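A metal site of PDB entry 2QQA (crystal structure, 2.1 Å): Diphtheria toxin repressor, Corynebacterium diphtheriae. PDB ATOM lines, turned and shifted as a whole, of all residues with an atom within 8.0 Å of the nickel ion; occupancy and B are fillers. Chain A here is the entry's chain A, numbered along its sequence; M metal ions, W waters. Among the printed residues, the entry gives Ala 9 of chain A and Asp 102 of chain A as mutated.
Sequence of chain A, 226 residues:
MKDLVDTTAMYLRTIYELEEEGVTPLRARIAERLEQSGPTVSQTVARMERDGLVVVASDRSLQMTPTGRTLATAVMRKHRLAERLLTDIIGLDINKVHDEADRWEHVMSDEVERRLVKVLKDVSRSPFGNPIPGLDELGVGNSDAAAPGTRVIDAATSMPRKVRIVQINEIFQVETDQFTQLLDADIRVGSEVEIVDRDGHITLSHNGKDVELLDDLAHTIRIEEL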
ATOM      1  N   ASP A   3      16.226 -14.018  -1.122  1.00  0.00           N
ATOM      2  CA  ASP A   3      15.048 -13.428  -0.413  1.00  0.00           C
ATOM      3  C   ASP A   3      13.851 -14.399  -0.393  1.00  0.00           C
ATOM      4  O   ASP A   3      13.033 -14.347   0.543  1.00  0.00           O
ATOM      5  CB  ASP A   3      14.653 -12.065  -1.018  1.00  0.00           C
ATOM      6  CG  ASP A   3      15.534 -11.682  -2.224  1.00  0.00           C
ATOM      7  OD1 ASP A   3      16.627 -11.113  -1.998  1.00  0.00           O
ATOM      8  OD2 ASP A   3      15.137 -11.946  -3.384  1.00  0.00           O
ATOM      9  N   LEU A   4      13.755 -15.264  -1.414  1.00  0.00           N
ATOM     10  CA  LEU A   4      12.638 -16.231  -1.572  1.00  0.00           C
ATOM     11  C   LEU A   4      12.706 -17.430  -0.592  1.00  0.00           C
ATOM     12  O   LEU A   4      11.695 -18.095  -0.389  1.00  0.00           O
ATOM     13  CB  LEU A   4      12.508 -16.694  -3.048  1.00  0.00           C
ATOM     14  CG  LEU A   4      11.901 -15.784  -4.167  1.00  0.00           C
ATOM     15  CD1 LEU A   4      11.702 -16.523  -5.447  1.00  0.00           C
ATOM     16  CD2 LEU A   4      10.567 -15.133  -3.711  1.00  0.00           C
ATOM     17  N   VAL A   5      13.900 -17.641  -0.005  1.00  0.00           N
ATOM     18  CA  VAL A   5      14.254 -18.668   0.997  1.00  0.00           C
ATOM     19  C   VAL A   5      14.310 -20.073   0.398  1.00  0.00           C
ATOM     20  O   VAL A   5      15.369 -20.720   0.363  1.00  0.00           O
ATOM     21  CB  VAL A   5      13.358 -18.574   2.299  1.00  0.00           C
ATOM     22  CG1 VAL A   5      13.712 -19.655   3.333  1.00  0.00           C
ATOM     23  CG2 VAL A   5      13.365 -17.132   2.904  1.00  0.00           C
ATOM     24  N   ASP A   6      13.143 -20.569  -0.059  1.00  0.00           N
ATOM     25  CA  ASP A   6      13.092 -21.801  -0.824  1.00  0.00           C
ATOM     26  C   ASP A   6      12.344 -21.468  -2.121  1.00  0.00           C
ATOM     27  O   ASP A   6      11.141 -21.296  -2.103  1.00  0.00           O
ATOM     28  CB  ASP A   6      12.343 -22.862  -0.031  1.00  0.00           C
ATOM     29  CG  ASP A   6      12.325 -24.221  -0.731  1.00  0.00           C
ATOM     30  OD1 ASP A   6      12.092 -25.219  -0.006  1.00  0.00           O
ATOM     31  OD2 ASP A   6      12.533 -24.305  -1.979  1.00  0.00           O
ATOM     32  N   THR A   7      13.056 -21.368  -3.233  1.00  0.00           N
ATOM     33  CA  THR A   7      12.447 -20.807  -4.413  1.00  0.00           C
ATOM     34  C   THR A   7      11.354 -21.784  -4.958  1.00  0.00           C
ATOM     35  O   THR A   7      10.248 -21.398  -5.207  1.00  0.00           O
ATOM     36  CB  THR A   7      13.499 -20.413  -5.477  1.00  0.00           C
ATOM     37  OG1 THR A   7      14.206 -21.558  -5.874  1.00  0.00           O
ATOM     38  CG2 THR A   7      14.566 -19.435  -4.914  1.00  0.00           C
ATOM     39  N   ALA A   9       9.588 -24.074  -3.368  1.00  0.00           N
ATOM     40  CA  ALA A   9       8.442 -24.071  -2.538  1.00  0.00           C
ATOM     41  C   ALA A   9       7.631 -22.837  -2.764  1.00  0.00           C
ATOM     42  O   ALA A   9       6.370 -22.920  -2.658  1.00  0.00           O
ATOM     43  CB  ALA A   9       8.867 -24.126  -1.079  1.00  0.00           C
ATOM     44  N   MET A  10       8.293 -21.686  -3.039  1.00  0.00           N
ATOM     45  CA  MET A  10       7.551 -20.402  -3.357  1.00  0.00           C
ATOM     46  C   MET A  10       6.761 -20.454  -4.666  1.00  0.00           C
ATOM     47  O   MET A  10       5.648 -19.995  -4.739  1.00  0.00           O
ATOM     48  CB  MET A  10       8.477 -19.231  -3.432  1.00  0.00           C
ATOM     49  CG  MET A  10       8.776 -18.731  -2.059  1.00  0.00           C
ATOM     50  SD  MET A  10       7.243 -18.320  -1.208  1.00  0.00           S
ATOM     51  CE  MET A  10       7.016 -16.579  -1.781  1.00  0.00           C
ATOM     52  N   TYR A  11       7.366 -20.992  -5.694  1.00  0.00           N
ATOM     53  CA  TYR A  11       6.618 -21.279  -6.918  1.00  0.00           C
ATOM     54  C   TYR A  11       5.377 -22.171  -6.675  1.00  0.00           C
ATOM     55  O   TYR A  11       4.330 -21.905  -7.206  1.00  0.00           O
ATOM     56  CB  TYR A  11       7.494 -21.882  -7.934  1.00  0.00           C
ATOM     57  CG  TYR A  11       8.382 -20.914  -8.697  1.00  0.00           C
ATOM     58  CD1 TYR A  11       9.316 -20.082  -8.029  1.00  0.00           C
ATOM     59  CD2 TYR A  11       8.401 -20.929 -10.086  1.00  0.00           C
ATOM     60  CE1 TYR A  11      10.175 -19.210  -8.741  1.00  0.00           C
ATOM     61  CE2 TYR A  11       9.272 -20.081 -10.824  1.00  0.00           C
ATOM     62  CZ  TYR A  11      10.167 -19.236 -10.124  1.00  0.00           C
ATOM     63  OH  TYR A  11      11.005 -18.385 -10.836  1.00  0.00           O
ATOM     64  N   ARG A  13       3.664 -22.678  -3.725  1.00  0.00           N
ATOM     65  CA  ARG A  13       2.720 -21.901  -2.947  1.00  0.00           C
ATOM     66  C   ARG A  13       1.955 -20.858  -3.773  1.00  0.00           C
ATOM     67  O   ARG A  13       0.770 -20.637  -3.556  1.00  0.00           O
ATOM     68  CB  ARG A  13       3.347 -21.202  -1.701  1.00  0.00           C
ATOM     69  CG  ARG A  13       2.211 -20.558  -0.776  1.00  0.00           C
ATOM     70  CD  ARG A  13       2.594 -19.395   0.278  1.00  0.00           C
ATOM     71  NE  ARG A  13       2.497 -18.077  -0.322  1.00  0.00           N
ATOM     72  CZ  ARG A  13       3.420 -17.137  -0.219  1.00  0.00           C
ATOM     73  NH1 ARG A  13       4.477 -17.325   0.564  1.00  0.00           N
ATOM     74  NH2 ARG A  13       3.270 -15.982  -0.903  1.00  0.00           N
ATOM     75  N   THR A  14       2.652 -20.248  -4.716  1.00  0.00           N
ATOM     76  CA  THR A  14       2.050 -19.290  -5.634  1.00  0.00           C
ATOM     77  C   THR A  14       1.089 -19.957  -6.659  1.00  0.00           C
ATOM     78  O   THR A  14      -0.011 -19.428  -6.908  1.00  0.00           O
ATOM     79  CB  THR A  14       3.152 -18.561  -6.408  1.00  0.00           C
ATOM     80  OG1 THR A  14       4.086 -17.936  -5.487  1.00  0.00           O
ATOM     81  CG2 THR A  14       2.512 -17.563  -7.373  1.00  0.00           C
ATOM     82  N   LEU A  34       5.650 -13.019  -7.838  1.00  0.00           N
ATOM     83  CA  LEU A  34       6.952 -13.167  -7.125  1.00  0.00           C
ATOM     84  C   LEU A  34       7.930 -12.081  -7.517  1.00  0.00           C
ATOM     85  O   LEU A  34       9.112 -12.108  -7.139  1.00  0.00           O
ATOM     86  CB  LEU A  34       7.574 -14.545  -7.471  1.00  0.00           C
ATOM     87  CG  LEU A  34       6.787 -15.742  -6.944  1.00  0.00           C
ATOM     88  CD1 LEU A  34       7.420 -17.067  -7.338  1.00  0.00           C
ATOM     89  CD2 LEU A  34       6.626 -15.610  -5.348  1.00  0.00           C
ATOM     90  N   VAL A  75       3.322 -26.523   2.335  1.00  0.00           N
ATOM     91  CA  VAL A  75       3.892 -25.196   2.436  1.00  0.00           C
ATOM     92  C   VAL A  75       2.777 -24.248   2.847  1.00  0.00           C
ATOM     93  O   VAL A  75       3.016 -23.422   3.704  1.00  0.00           O
ATOM     94  CB  VAL A  75       4.556 -24.680   1.174  1.00  0.00           C
ATOM     95  CG1 VAL A  75       5.030 -23.236   1.404  1.00  0.00           C
ATOM     96  CG2 VAL A  75       5.808 -25.537   0.858  1.00  0.00           C
ATOM     97  N   HIS A  79       2.439 -22.041   6.160  1.00  0.00           N
ATOM     98  CA  HIS A  79       2.310 -20.593   5.990  1.00  0.00           C
ATOM     99  C   HIS A  79       1.158 -19.906   6.770  1.00  0.00           C
ATOM    100  O   HIS A  79       1.348 -18.900   7.467  1.00  0.00           O
ATOM    101  CB  HIS A  79       2.196 -20.312   4.501  1.00  0.00           C
ATOM    102  CG  HIS A  79       2.002 -18.881   4.219  1.00  0.00           C
ATOM    103  ND1 HIS A  79       3.039 -17.985   4.250  1.00  0.00           N
ATOM    104  CD2 HIS A  79       0.892 -18.176   3.929  1.00  0.00           C
ATOM    105  CE1 HIS A  79       2.583 -16.776   3.945  1.00  0.00           C
ATOM    106  NE2 HIS A  79       1.281 -16.865   3.767  1.00  0.00           N
ATOM    107  N   HIS A  98       2.206 -11.422   6.903  1.00  0.00           N
ATOM    108  CA  HIS A  98       2.265 -12.318   5.750  1.00  0.00           C
ATOM    109  C   HIS A  98       3.749 -12.417   5.331  1.00  0.00           C
ATOM    110  O   HIS A  98       4.231 -13.490   4.994  1.00  0.00           O
ATOM    111  CB  HIS A  98       1.376 -11.930   4.541  1.00  0.00           C
ATOM    112  CG  HIS A  98       1.941 -12.429   3.249  1.00  0.00           C
ATOM    113  ND1 HIS A  98       1.732 -13.717   2.800  1.00  0.00           N
ATOM    114  CD2 HIS A  98       2.817 -11.860   2.384  1.00  0.00           C
ATOM    115  CE1 HIS A  98       2.410 -13.897   1.683  1.00  0.00           C
ATOM    116  NE2 HIS A  98       3.115 -12.798   1.434  1.00  0.00           N
ATOM    117  N   ASP A  99       4.459 -11.271   5.385  1.00  0.00           N
ATOM    118  CA  ASP A  99       5.842 -11.211   4.881  1.00  0.00           C
ATOM    119  C   ASP A  99       6.728 -12.058   5.827  1.00  0.00           C
ATOM    120  O   ASP A  99       7.627 -12.725   5.381  1.00  0.00           O
ATOM    121  CB  ASP A  99       6.369  -9.787   4.875  1.00  0.00           C
ATOM    122  CG  ASP A  99       5.918  -8.963   3.658  1.00  0.00           C
ATOM    123  OD1 ASP A  99       5.463  -9.458   2.545  1.00  0.00           O
ATOM    124  OD2 ASP A  99       6.049  -7.730   3.851  1.00  0.00           O
ATOM    125  N   GLU A 100       6.445 -12.020   7.137  1.00  0.00           N
ATOM    126  CA  GLU A 100       7.148 -12.913   8.087  1.00  0.00           C
ATOM    127  C   GLU A 100       6.813 -14.402   7.768  1.00  0.00           C
ATOM    128  O   GLU A 100       7.689 -15.251   7.617  1.00  0.00           O
ATOM    129  CB  GLU A 100       6.796 -12.521   9.518  1.00  0.00           C
ATOM    130  CG  GLU A 100       7.666 -13.138  10.550  1.00  0.00           C
ATOM    131  CD  GLU A 100       8.939 -12.371  10.764  1.00  0.00           C
ATOM    132  OE1 GLU A 100       9.907 -13.034  11.181  1.00  0.00           O
ATOM    133  OE2 GLU A 100       8.952 -11.102  10.610  1.00  0.00           O
ATOM    134  N   ALA A 101       5.536 -14.729   7.612  1.00  0.00           N
ATOM    135  CA  ALA A 101       5.157 -16.106   7.371  1.00  0.00           C
ATOM    136  C   ALA A 101       5.680 -16.617   6.036  1.00  0.00           C
ATOM    137  O   ALA A 101       5.923 -17.811   5.871  1.00  0.00           O
ATOM    138  CB  ALA A 101       3.669 -16.263   7.515  1.00  0.00           C
ATOM    139  N   ASP A 102       5.895 -15.700   5.104  1.00  0.00           N
ATOM    140  CA  ASP A 102       6.415 -16.003   3.792  1.00  0.00           C
ATOM    141  C   ASP A 102       7.859 -16.577   4.019  1.00  0.00           C
ATOM    142  O   ASP A 102       8.276 -17.390   3.297  1.00  0.00           O
ATOM    143  CB  ASP A 102       6.496 -14.664   3.048  1.00  0.00           C
ATOM    144  CG  ASP A 102       6.659 -14.795   1.569  1.00  0.00           C
ATOM    145  OD1 ASP A 102       6.755 -13.737   0.908  1.00  0.00           O
ATOM    146  OD2 ASP A 102       6.720 -15.890   0.987  1.00  0.00           O
ATOM    147  N   ARG A 103       8.610 -16.124   5.035  1.00  0.00           N
ATOM    148  CA  ARG A 103       9.910 -16.771   5.324  1.00  0.00           C
ATOM    149  C   ARG A 103       9.791 -18.030   6.182  1.00  0.00           C
ATOM    150  O   ARG A 103      10.441 -19.048   5.891  1.00  0.00           O
ATOM    151  CB  ARG A 103      10.871 -15.747   5.914  1.00  0.00           C
ATOM    152  CG  ARG A 103      11.149 -14.578   4.937  1.00  0.00           C
ATOM    153  CD  ARG A 103      12.360 -13.819   5.459  1.00  0.00           C
ATOM    154  NE  ARG A 103      12.041 -13.295   6.772  1.00  0.00           N
ATOM    155  CZ  ARG A 103      11.278 -12.215   7.007  1.00  0.00           C
ATOM    156  NH1 ARG A 103      10.724 -11.479   6.025  1.00  0.00           N
ATOM    157  NH2 ARG A 103      11.020 -11.876   8.225  1.00  0.00           N
ATOM    158  N   TRP A 104       8.950 -17.972   7.214  1.00  0.00           N
ATOM    159  CA  TRP A 104       8.810 -19.046   8.197  1.00  0.00           C
ATOM    160  C   TRP A 104       8.322 -20.358   7.587  1.00  0.00           C
ATOM    161  O   TRP A 104       8.646 -21.422   8.076  1.00  0.00           O
ATOM    162  CB  TRP A 104       7.923 -18.632   9.404  1.00  0.00           C
ATOM    163  CG  TRP A 104       8.517 -17.565  10.289  1.00  0.00           C
ATOM    164  CD1 TRP A 104       9.452 -16.607   9.943  1.00  0.00           C
ATOM    165  CD2 TRP A 104       8.190 -17.335  11.669  1.00  0.00           C
ATOM    166  NE1 TRP A 104       9.737 -15.823  11.042  1.00  0.00           N
ATOM    167  CE2 TRP A 104       8.990 -16.249  12.115  1.00  0.00           C
ATOM    168  CE3 TRP A 104       7.319 -17.963  12.595  1.00  0.00           C
ATOM    169  CZ2 TRP A 104       8.906 -15.736  13.420  1.00  0.00           C
ATOM    170  CZ3 TRP A 104       7.253 -17.452  13.876  1.00  0.00           C
ATOM    171  CH2 TRP A 104       8.055 -16.364  14.286  1.00  0.00           C
ATOM    172  N   GLU A 105       7.533 -20.268   6.540  1.00  0.00           N
ATOM    173  CA  GLU A 105       6.874 -21.440   5.946  1.00  0.00           C
ATOM    174  C   GLU A 105       7.872 -22.479   5.380  1.00  0.00           C
ATOM    175  O   GLU A 105       7.520 -23.643   5.275  1.00  0.00           O
ATOM    176  CB  GLU A 105       5.898 -21.054   4.822  1.00  0.00           C
ATOM    177  CG  GLU A 105       6.638 -20.500   3.564  1.00  0.00           C
ATOM    178  CD  GLU A 105       5.623 -19.846   2.580  1.00  0.00           C
ATOM    179  OE1 GLU A 105       4.445 -20.071   2.704  1.00  0.00           O
ATOM    180  OE2 GLU A 105       5.987 -19.132   1.698  1.00  0.00           O
ATOM    181  N   HIS A 106       9.075 -22.028   5.034  1.00  0.00           N
ATOM    182  CA  HIS A 106      10.097 -22.846   4.435  1.00  0.00           C
ATOM    183  C   HIS A 106      10.948 -23.518   5.561  1.00  0.00           C
ATOM    184  O   HIS A 106      11.718 -24.460   5.290  1.00  0.00           O
ATOM    185  CB  HIS A 106      10.953 -21.929   3.526  1.00  0.00           C
ATOM    186  CG  HIS A 106      10.146 -21.208   2.478  1.00  0.00           C
ATOM    187  ND1 HIS A 106       9.404 -21.871   1.533  1.00  0.00           N
ATOM    188  CD2 HIS A 106       9.904 -19.891   2.262  1.00  0.00           C
ATOM    189  CE1 HIS A 106       8.791 -21.011   0.745  1.00  0.00           C
ATOM    190  NE2 HIS A 106       9.113 -19.803   1.151  1.00  0.00           N
HETATM  191 NI    NI M   1       7.831 -17.903   1.270  1.00  0.00          NI
HETATM  192  O   HOH W   1       9.624 -16.954   0.468  1.00  0.00           O
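NH1 of Arg 13 sits close to OD2 of Asp 102 (2.7 Å).
OE1 of Glu 105 lies within salt-bridge range of NH1 of Arg 13 (3.5 Å).
The side-chain carboxylate (OE1) of Glu 105 sits close to a ring nitrogen (ND1) of His 79 (3.0 Å).
The backbone carbonyl oxygen of Leu 4 sits close to a ring nitrogen (NE2) of His 106 (3.5 Å).
SD of Met 10 lies close to NH1 of Arg 13 (3.4 Å).
The side-chain hydroxyl of Thr 14 is in hydrogen-bond range of the backbone carbonyl oxygen of Met 10.
Arg 13 touches the nickel ion (NH1 to NI, 3.5 Å).
Five residues have an atom within 4 Å of the nickel ion: Met 10, Arg 13, Asp 102, Glu 105 and His 106.
The nearest printed residue that does not touch the nickel ion is Leu 4 (4.2 Å).
The nickel ion is bound by O of Asp 102 (2.1 Å), water W1 (2.2 Å), OE2 of Glu 105 (2.3 Å), NE2 of His 106 (2.3 Å), OD2 of Asp 102 (2.3 Å) and SD of Met 10 (2.6 Å).
The nickel ion has six donor atoms within binding distance.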
